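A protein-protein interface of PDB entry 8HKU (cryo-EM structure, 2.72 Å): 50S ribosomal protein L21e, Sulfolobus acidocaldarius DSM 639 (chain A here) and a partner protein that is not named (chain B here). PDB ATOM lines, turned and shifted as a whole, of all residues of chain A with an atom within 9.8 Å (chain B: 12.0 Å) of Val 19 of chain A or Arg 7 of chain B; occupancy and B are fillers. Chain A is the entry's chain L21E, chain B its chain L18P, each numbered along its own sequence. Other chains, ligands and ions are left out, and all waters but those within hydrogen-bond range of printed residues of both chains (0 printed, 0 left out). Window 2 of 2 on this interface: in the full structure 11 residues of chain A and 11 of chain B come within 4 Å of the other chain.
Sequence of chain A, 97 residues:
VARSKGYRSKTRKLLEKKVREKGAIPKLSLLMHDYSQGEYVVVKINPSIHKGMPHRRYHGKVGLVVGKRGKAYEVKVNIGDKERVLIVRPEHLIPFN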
ATOM      1  N   GLU A  16      34.023  -7.232  18.254  1.00  0.00           N
ATOM      2  CA  GLU A  16      34.257  -8.002  17.047  1.00  0.00           C
ATOM      3  C   GLU A  16      33.773  -9.428  17.213  1.00  0.00           C
ATOM      4  O   GLU A  16      33.535  -9.920  18.316  1.00  0.00           O
ATOM      5  CB  GLU A  16      35.732  -8.068  16.677  1.00  0.00           C
ATOM      6  CG  GLU A  16      36.392  -6.809  16.261  1.00  0.00           C
ATOM      7  CD  GLU A  16      35.851  -6.306  14.961  1.00  0.00           C
ATOM      8  OE1 GLU A  16      35.449  -7.142  14.134  1.00  0.00           O
ATOM      9  OE2 GLU A  16      35.906  -5.089  14.725  1.00  0.00           O
ATOM     10  N   LYS A  17      33.650 -10.092  16.081  1.00  0.00           N
ATOM     11  CA  LYS A  17      33.314 -11.497  16.009  1.00  0.00           C
ATOM     12  C   LYS A  17      34.277 -12.136  15.022  1.00  0.00           C
ATOM     13  O   LYS A  17      34.508 -11.592  13.941  1.00  0.00           O
ATOM     14  CB  LYS A  17      31.857 -11.651  15.581  1.00  0.00           C
ATOM     15  CG  LYS A  17      31.297 -13.014  15.758  1.00  0.00           C
ATOM     16  CD  LYS A  17      29.794 -12.976  15.780  1.00  0.00           C
ATOM     17  CE  LYS A  17      29.292 -12.872  17.186  1.00  0.00           C
ATOM     18  NZ  LYS A  17      27.907 -13.370  17.257  1.00  0.00           N
ATOM     19  N   LYS A  18      34.878 -13.260  15.403  1.00  0.00           N
ATOM     20  CA  LYS A  18      35.819 -13.911  14.504  1.00  0.00           C
ATOM     21  C   LYS A  18      35.088 -14.588  13.350  1.00  0.00           C
ATOM     22  O   LYS A  18      33.905 -14.907  13.432  1.00  0.00           O
ATOM     23  CB  LYS A  18      36.677 -14.928  15.249  1.00  0.00           C
ATOM     24  CG  LYS A  18      38.028 -14.381  15.665  1.00  0.00           C
ATOM     25  CD  LYS A  18      38.712 -15.298  16.654  1.00  0.00           C
ATOM     26  CE  LYS A  18      37.835 -15.533  17.861  1.00  0.00           C
ATOM     27  NZ  LYS A  18      38.434 -16.467  18.850  1.00  0.00           N
ATOM     28  N   VAL A  19      35.827 -14.823  12.265  1.00  0.00           N
ATOM     29  CA  VAL A  19      35.219 -15.214  10.995  1.00  0.00           C
ATOM     30  C   VAL A  19      34.431 -16.510  11.120  1.00  0.00           C
ATOM     31  O   VAL A  19      33.488 -16.744  10.359  1.00  0.00           O
ATOM     32  CB  VAL A  19      36.306 -15.308   9.904  1.00  0.00           C
ATOM     33  CG1 VAL A  19      37.317 -16.370  10.257  1.00  0.00           C
ATOM     34  CG2 VAL A  19      35.688 -15.592   8.554  1.00  0.00           C
ATOM     35  N   ARG A  20      34.779 -17.358  12.079  1.00  0.00           N
ATOM     36  CA  ARG A  20      34.121 -18.642  12.253  1.00  0.00           C
ATOM     37  C   ARG A  20      33.115 -18.651  13.394  1.00  0.00           C
ATOM     38  O   ARG A  20      32.694 -19.727  13.824  1.00  0.00           O
ATOM     39  CB  ARG A  20      35.161 -19.734  12.474  1.00  0.00           C
ATOM     40  CG  ARG A  20      35.642 -20.368  11.199  1.00  0.00           C
ATOM     41  CD  ARG A  20      36.436 -21.601  11.498  1.00  0.00           C
ATOM     42  NE  ARG A  20      37.137 -22.088  10.319  1.00  0.00           N
ATOM     43  CZ  ARG A  20      37.733 -23.266  10.246  1.00  0.00           C
ATOM     44  NH1 ARG A  20      37.720 -24.111  11.260  1.00  0.00           N
ATOM     45  NH2 ARG A  20      38.357 -23.605   9.127  1.00  0.00           N
ATOM     46  N   GLU A  21      32.727 -17.488  13.902  1.00  0.00           N
ATOM     47  CA  GLU A  21      31.660 -17.399  14.884  1.00  0.00           C
ATOM     48  C   GLU A  21      30.501 -16.535  14.427  1.00  0.00           C
ATOM     49  O   GLU A  21      29.536 -16.376  15.177  1.00  0.00           O
ATOM     50  CB  GLU A  21      32.190 -16.859  16.211  1.00  0.00           C
ATOM     51  CG  GLU A  21      33.554 -17.360  16.557  1.00  0.00           C
ATOM     52  CD  GLU A  21      34.016 -16.836  17.885  1.00  0.00           C
ATOM     53  OE1 GLU A  21      33.161 -16.368  18.664  1.00  0.00           O
ATOM     54  OE2 GLU A  21      35.226 -16.919  18.165  1.00  0.00           O
ATOM     55  N   LYS A  22      30.562 -15.988  13.224  1.00  0.00           N
ATOM     56  CA  LYS A  22      29.514 -15.118  12.740  1.00  0.00           C
ATOM     57  C   LYS A  22      28.247 -15.908  12.430  1.00  0.00           C
ATOM     58  O   LYS A  22      28.270 -17.123  12.225  1.00  0.00           O
ATOM     59  CB  LYS A  22      29.993 -14.369  11.503  1.00  0.00           C
ATOM     60  CG  LYS A  22      31.169 -13.478  11.782  1.00  0.00           C
ATOM     61  CD  LYS A  22      31.438 -12.533  10.642  1.00  0.00           C
ATOM     62  CE  LYS A  22      32.420 -11.473  11.080  1.00  0.00           C
ATOM     63  NZ  LYS A  22      32.629 -10.443  10.042  1.00  0.00           N
ATOM     64  N   GLY A  23      27.130 -15.196  12.412  1.00  0.00           N
ATOM     65  CA  GLY A  23      25.829 -15.742  12.101  1.00  0.00           C
ATOM     66  C   GLY A  23      24.918 -15.759  13.314  1.00  0.00           C
ATOM     67  O   GLY A  23      25.358 -15.753  14.465  1.00  0.00           O
ATOM     68  N   ALA A  24      23.616 -15.796  13.037  1.00  0.00           N
ATOM     69  CA  ALA A  24      22.617 -15.823  14.099  1.00  0.00           C
ATOM     70  C   ALA A  24      22.752 -17.099  14.925  1.00  0.00           C
ATOM     71  O   ALA A  24      23.006 -18.182  14.394  1.00  0.00           O
ATOM     72  CB  ALA A  24      21.218 -15.706  13.511  1.00  0.00           C
ATOM     73  N   ILE A  25      22.492 -16.971  16.226  1.00  0.00           N
ATOM     74  CA  ILE A  25      23.202 -17.707  17.277  1.00  0.00           C
ATOM     75  C   ILE A  25      23.546 -19.136  16.883  1.00  0.00           C
ATOM     76  O   ILE A  25      22.664 -19.917  16.505  1.00  0.00           O
ATOM     77  CB  ILE A  25      22.417 -17.702  18.594  1.00  0.00           C
ATOM     78  CG1 ILE A  25      23.077 -18.651  19.583  1.00  0.00           C
ATOM     79  CG2 ILE A  25      20.990 -18.079  18.365  1.00  0.00           C
ATOM     80  CD1 ILE A  25      22.621 -18.429  20.979  1.00  0.00           C
ATOM     81  N   PRO A  26      24.827 -19.488  16.902  1.00  0.00           N
ATOM     82  CA  PRO A  26      25.238 -20.849  16.542  1.00  0.00           C
ATOM     83  C   PRO A  26      25.026 -21.901  17.627  1.00  0.00           C
ATOM     84  O   PRO A  26      24.568 -23.007  17.323  1.00  0.00           O
ATOM     85  CB  PRO A  26      26.729 -20.684  16.212  1.00  0.00           C
ATOM     86  CG  PRO A  26      27.166 -19.509  16.990  1.00  0.00           C
ATOM     87  CD  PRO A  26      25.978 -18.593  17.109  1.00  0.00           C
ATOM     88  N   THR B   1      34.021 -23.289  -1.218  1.00  0.00           N
ATOM     89  CA  THR B   1      35.024 -22.856  -0.256  1.00  0.00           C
ATOM     90  C   THR B   1      36.218 -22.234  -0.935  1.00  0.00           C
ATOM     91  O   THR B   1      36.671 -22.712  -1.969  1.00  0.00           O
ATOM     92  CB  THR B   1      35.506 -24.012   0.598  1.00  0.00           C
ATOM     93  OG1 THR B   1      36.005 -25.051  -0.253  1.00  0.00           O
ATOM     94  CG2 THR B   1      34.378 -24.536   1.424  1.00  0.00           C
ATOM     95  N   GLN B   2      36.742 -21.165  -0.350  1.00  0.00           N
ATOM     96  CA  GLN B   2      37.835 -20.459  -0.993  1.00  0.00           C
ATOM     97  C   GLN B   2      38.968 -20.065  -0.061  1.00  0.00           C
ATOM     98  O   GLN B   2      39.975 -19.543  -0.547  1.00  0.00           O
ATOM     99  CB  GLN B   2      37.304 -19.206  -1.704  1.00  0.00           C
ATOM    100  CG  GLN B   2      36.377 -19.520  -2.863  1.00  0.00           C
ATOM    101  CD  GLN B   2      37.109 -20.151  -4.028  1.00  0.00           C
ATOM    102  OE1 GLN B   2      38.219 -19.748  -4.371  1.00  0.00           O
ATOM    103  NE2 GLN B   2      36.495 -21.158  -4.637  1.00  0.00           N
ATOM    104  N   GLY B   3      38.861 -20.291   1.240  1.00  0.00           N
ATOM    105  CA  GLY B   3      39.982 -20.021   2.101  1.00  0.00           C
ATOM    106  C   GLY B   3      39.614 -19.598   3.501  1.00  0.00           C
ATOM    107  O   GLY B   3      38.665 -20.100   4.105  1.00  0.00           O
ATOM    108  N   PRO B   4      40.388 -18.664   4.055  1.00  0.00           N
ATOM    109  CA  PRO B   4      40.221 -18.291   5.461  1.00  0.00           C
ATOM    110  C   PRO B   4      39.105 -17.295   5.730  1.00  0.00           C
ATOM    111  O   PRO B   4      38.876 -16.962   6.895  1.00  0.00           O
ATOM    112  CB  PRO B   4      41.586 -17.687   5.801  1.00  0.00           C
ATOM    113  CG  PRO B   4      42.038 -17.090   4.529  1.00  0.00           C
ATOM    114  CD  PRO B   4      41.526 -17.969   3.431  1.00  0.00           C
ATOM    115  N   ASN B   5      38.417 -16.800   4.705  1.00  0.00           N
ATOM    116  CA  ASN B   5      37.302 -15.881   4.881  1.00  0.00           C
ATOM    117  C   ASN B   5      35.948 -16.550   4.705  1.00  0.00           C
ATOM    118  O   ASN B   5      34.928 -15.858   4.684  1.00  0.00           O
ATOM    119  CB  ASN B   5      37.417 -14.717   3.903  1.00  0.00           C
ATOM    120  CG  ASN B   5      37.996 -13.483   4.534  1.00  0.00           C
ATOM    121  OD1 ASN B   5      37.990 -13.328   5.752  1.00  0.00           O
ATOM    122  ND2 ASN B   5      38.488 -12.581   3.705  1.00  0.00           N
ATOM    123  N   TYR B   6      35.913 -17.869   4.568  1.00  0.00           N
ATOM    124  CA  TYR B   6      34.693 -18.604   4.276  1.00  0.00           C
ATOM    125  C   TYR B   6      34.148 -19.222   5.551  1.00  0.00           C
ATOM    126  O   TYR B   6      34.892 -19.854   6.304  1.00  0.00           O
ATOM    127  CB  TYR B   6      34.969 -19.694   3.248  1.00  0.00           C
ATOM    128  CG  TYR B   6      33.765 -20.157   2.480  1.00  0.00           C
ATOM    129  CD1 TYR B   6      33.376 -19.518   1.321  1.00  0.00           C
ATOM    130  CD2 TYR B   6      33.028 -21.246   2.905  1.00  0.00           C
ATOM    131  CE1 TYR B   6      32.286 -19.939   0.614  1.00  0.00           C
ATOM    132  CE2 TYR B   6      31.937 -21.672   2.206  1.00  0.00           C
ATOM    133  CZ  TYR B   6      31.570 -21.018   1.060  1.00  0.00           C
ATOM    134  OH  TYR B   6      30.473 -21.444   0.354  1.00  0.00           O
ATOM    135  N   ARG B   7      32.853 -19.049   5.783  1.00  0.00           N
ATOM    136  CA  ARG B   7      32.172 -19.643   6.923  1.00  0.00           C
ATOM    137  C   ARG B   7      31.208 -20.716   6.439  1.00  0.00           C
ATOM    138  O   ARG B   7      30.383 -20.464   5.559  1.00  0.00           O
ATOM    139  CB  ARG B   7      31.427 -18.585   7.728  1.00  0.00           C
ATOM    140  CG  ARG B   7      31.100 -19.016   9.134  1.00  0.00           C
ATOM    141  CD  ARG B   7      30.191 -18.014   9.790  1.00  0.00           C
ATOM    142  NE  ARG B   7      28.785 -18.288   9.523  1.00  0.00           N
ATOM    143  CZ  ARG B   7      27.959 -17.458   8.900  1.00  0.00           C
ATOM    144  NH1 ARG B   7      28.369 -16.289   8.437  1.00  0.00           N
ATOM    145  NH2 ARG B   7      26.690 -17.814   8.732  1.00  0.00           N
ATOM    146  N   ILE B   8      31.316 -21.902   7.020  1.00  0.00           N
ATOM    147  CA  ILE B   8      30.510 -23.055   6.637  1.00  0.00           C
ATOM    148  C   ILE B   8      29.216 -23.045   7.432  1.00  0.00           C
ATOM    149  O   ILE B   8      29.226 -22.822   8.647  1.00  0.00           O
ATOM    150  CB  ILE B   8      31.288 -24.361   6.860  1.00  0.00           C
ATOM    151  CG1 ILE B   8      32.559 -24.345   6.037  1.00  0.00           C
ATOM    152  CG2 ILE B   8      30.486 -25.551   6.461  1.00  0.00           C
ATOM    153  CD1 ILE B   8      32.295 -24.245   4.569  1.00  0.00           C
ATOM    154  N   LYS B   9      28.100 -23.276   6.744  1.00  0.00           N
ATOM    155  CA  LYS B   9      26.808 -23.344   7.403  1.00  0.00           C
ATOM    156  C   LYS B   9      26.691 -24.637   8.198  1.00  0.00           C
ATOM    157  O   LYS B   9      27.502 -25.552   8.069  1.00  0.00           O
ATOM    158  CB  LYS B   9      25.685 -23.242   6.381  1.00  0.00           C
ATOM    159  CG  LYS B   9      25.565 -21.882   5.754  1.00  0.00           C
ATOM    160  CD  LYS B   9      24.368 -21.800   4.832  1.00  0.00           C
ATOM    161  CE  LYS B   9      24.240 -20.407   4.247  1.00  0.00           C
ATOM    162  NZ  LYS B   9      23.107 -20.299   3.293  1.00  0.00           N
ATOM    163  N   PHE B  10      25.663 -24.708   9.036  1.00  0.00           N
ATOM    164  CA  PHE B  10      25.472 -25.891   9.859  1.00  0.00           C
ATOM    165  C   PHE B  10      25.218 -27.107   8.981  1.00  0.00           C
ATOM    166  O   PHE B  10      24.747 -26.995   7.849  1.00  0.00           O
ATOM    167  CB  PHE B  10      24.314 -25.688  10.831  1.00  0.00           C
ATOM    168  CG  PHE B  10      24.651 -24.820  12.001  1.00  0.00           C
ATOM    169  CD1 PHE B  10      25.896 -24.235  12.112  1.00  0.00           C
ATOM    170  CD2 PHE B  10      23.727 -24.594  12.997  1.00  0.00           C
ATOM    171  CE1 PHE B  10      26.201 -23.438  13.186  1.00  0.00           C
ATOM    172  CE2 PHE B  10      24.032 -23.804  14.070  1.00  0.00           C
ATOM    173  CZ  PHE B  10      25.268 -23.228  14.163  1.00  0.00           C
ATOM    174  N   ARG B  11      25.564 -28.283   9.503  1.00  0.00           N
ATOM    175  CA  ARG B  11      25.513 -29.487   8.683  1.00  0.00           C
ATOM    176  C   ARG B  11      24.093 -29.803   8.239  1.00  0.00           C
ATOM    177  O   ARG B  11      23.857 -30.098   7.065  1.00  0.00           O
ATOM    178  CB  ARG B  11      26.112 -30.665   9.440  1.00  0.00           C
ATOM    179  CG  ARG B  11      26.079 -31.943   8.656  1.00  0.00           C
ATOM    180  CD  ARG B  11      26.764 -33.055   9.393  1.00  0.00           C
ATOM    181  NE  ARG B  11      26.153 -33.348  10.681  1.00  0.00           N
ATOM    182  CZ  ARG B  11      25.076 -34.098  10.839  1.00  0.00           C
ATOM    183  NH1 ARG B  11      24.412 -34.578   9.806  1.00  0.00           N
ATOM    184  NH2 ARG B  11      24.651 -34.372  12.067  1.00  0.00           N
ATOM    185  N   ARG B  13      21.718 -27.665   8.013  1.00  0.00           N
ATOM    186  CA  ARG B  13      21.273 -26.608   7.114  1.00  0.00           C
ATOM    187  C   ARG B  13      21.811 -26.827   5.708  1.00  0.00           C
ATOM    188  O   ARG B  13      21.125 -26.542   4.723  1.00  0.00           O
ATOM    189  CB  ARG B  13      21.700 -25.246   7.655  1.00  0.00           C
ATOM    190  CG  ARG B  13      21.535 -24.095   6.685  1.00  0.00           C
ATOM    191  CD  ARG B  13      20.091 -23.831   6.351  1.00  0.00           C
ATOM    192  NE  ARG B  13      19.962 -22.769   5.363  1.00  0.00           N
ATOM    193  CZ  ARG B  13      19.804 -22.971   4.064  1.00  0.00           C
ATOM    194  NH1 ARG B  13      19.702 -24.187   3.563  1.00  0.00           N
ATOM    195  NH2 ARG B  13      19.741 -21.925   3.249  1.00  0.00           N
ATOM    196  N   ARG B  14      23.040 -27.334   5.595  1.00  0.00           N
ATOM    197  CA  ARG B  14      23.595 -27.655   4.285  1.00  0.00           C
ATOM    198  C   ARG B  14      22.823 -28.780   3.614  1.00  0.00           C
ATOM    199  O   ARG B  14      22.595 -28.747   2.402  1.00  0.00           O
ATOM    200  CB  ARG B  14      25.063 -28.040   4.419  1.00  0.00           C
ATOM    201  CG  ARG B  14      26.016 -26.879   4.374  1.00  0.00           C
ATOM    202  CD  ARG B  14      27.446 -27.371   4.332  1.00  0.00           C
ATOM    203  NE  ARG B  14      27.908 -27.804   5.642  1.00  0.00           N
ATOM    204  CZ  ARG B  14      28.262 -29.044   5.932  1.00  0.00           C
ATOM    205  NH1 ARG B  14      28.229 -30.001   5.024  1.00  0.00           N
ATOM    206  NH2 ARG B  14      28.666 -29.331   7.164  1.00  0.00           N
ATOM    207  N   TYR B  20      16.898 -23.763  11.756  1.00  0.00           N
ATOM    208  CA  TYR B  20      17.457 -23.413  13.051  1.00  0.00           C
ATOM    209  C   TYR B  20      16.889 -22.128  13.622  1.00  0.00           C
ATOM    210  O   TYR B  20      17.113 -21.847  14.801  1.00  0.00           O
ATOM    211  CB  TYR B  20      18.977 -23.308  12.948  1.00  0.00           C
ATOM    212  CG  TYR B  20      19.658 -24.647  12.974  1.00  0.00           C
ATOM    213  CD1 TYR B  20      19.907 -25.285  14.167  1.00  0.00           C
ATOM    214  CD2 TYR B  20      20.029 -25.277  11.807  1.00  0.00           C
ATOM    215  CE1 TYR B  20      20.507 -26.506  14.200  1.00  0.00           C
ATOM    216  CE2 TYR B  20      20.642 -26.499  11.832  1.00  0.00           C
ATOM    217  CZ  TYR B  20      20.876 -27.109  13.032  1.00  0.00           C
ATOM    218  OH  TYR B  20      21.488 -28.331  13.067  1.00  0.00           O
ATOM    219  N   TYR B  21      16.176 -21.339  12.824  1.00  0.00           N
ATOM    220  CA  TYR B  21      15.525 -20.154  13.362  1.00  0.00           C
ATOM    221  C   TYR B  21      14.320 -20.526  14.208  1.00  0.00           C
ATOM    222  O   TYR B  21      14.082 -19.921  15.256  1.00  0.00           O
ATOM    223  CB  TYR B  21      15.133 -19.229  12.223  1.00  0.00           C
ATOM    224  CG  TYR B  21      16.324 -18.768  11.444  1.00  0.00           C
ATOM    225  CD1 TYR B  21      17.125 -17.750  11.917  1.00  0.00           C
ATOM    226  CD2 TYR B  21      16.663 -19.363  10.245  1.00  0.00           C
ATOM    227  CE1 TYR B  21      18.222 -17.329  11.216  1.00  0.00           C
ATOM    228  CE2 TYR B  21      17.757 -18.947   9.534  1.00  0.00           C
ATOM    229  CZ  TYR B  21      18.534 -17.930  10.025  1.00  0.00           C
ATOM    230  OH  TYR B  21      19.632 -17.508   9.323  1.00  0.00           O
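The guanidinium group of Arg 7 of chain B lies within hydrogen-bond range of the backbone carbonyl oxygen of Lys 22 of chain A, at 3.0 Å.
Val 19 of chain A touches Pro 4 of chain B.
CG2 of Val 19 of chain A touches O of Asn 5 of chain B, at 3.95 Å.
CG of Arg 7 of chain B touches O of Val 19 of chain A, at 3.5 Å.
Pro 26 of chain A touches Phe 10 of chain B (O to CZ, 3.2 Å).
Val 19 of chain A touches just these residues of chain B: Pro 4 (3.8 Å), Asn 5 (3.95 Å) and Arg 7 (3.5 Å).
Of chain A, only Val 19 and Lys 22 come within 4 Å of Arg 7 of chain B.
No residue of chain B comes within 4 Å of Lys 18 of chain A.
No residue of chain B comes within 4 Å of Arg 20 of chain A.
Of chain B, only Arg 7 (3.0 Å) comes within 4 Å of Lys 22 of chain A.
Gly 23 of chain A touches none of the printed residues of chain B.
No residue of chain B comes within 4 Å of Ala 24 of chain A.
No residue of chain A comes within 4 Å of Tyr 6 of chain B.
Of the printed residues of chain A, Pro 4 of chain B touches Val 19.
Of the printed residues of chain A, Phe 10 of chain B touches Pro 26 (3.2 Å).
Printed residues of chain A within 4 Å of Asn 5 of chain B: Val 19 (3.95 Å).
Printed residues of chain B within 4 Å of Pro 26 of chain A: Phe 10 (3.2 Å).
Ile 25 of chain A touches none of the printed residues of chain B.
Arg 11 of chain B touches none of the printed residues of chain A.
The nearest residue of chain B that does not touch Val 19 of chain A is Tyr 6 of chain B (4.6 Å).
The nearest residue of chain A that does not touch Arg 7 of chain B is Gly 23 of chain A (4.05 Å).
The nearest printed residue of chain A that does not touch Asn 5 of chain B is Lys 22 of chain A (7.4 Å).
Of the 15 printed residues of chain B, 4 touch a printed residue of chain A.
Hydrophobic or aromatic side chains of chain B within 4 Å of the printed part of chain A: Phe 10.
Of the 11 printed residues of chain A, 3 touch a printed residue of chain B.
Hydrophobic or aromatic side chains of chain A within 4 Å of the printed part of chain B: Val 19 and Pro 26.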
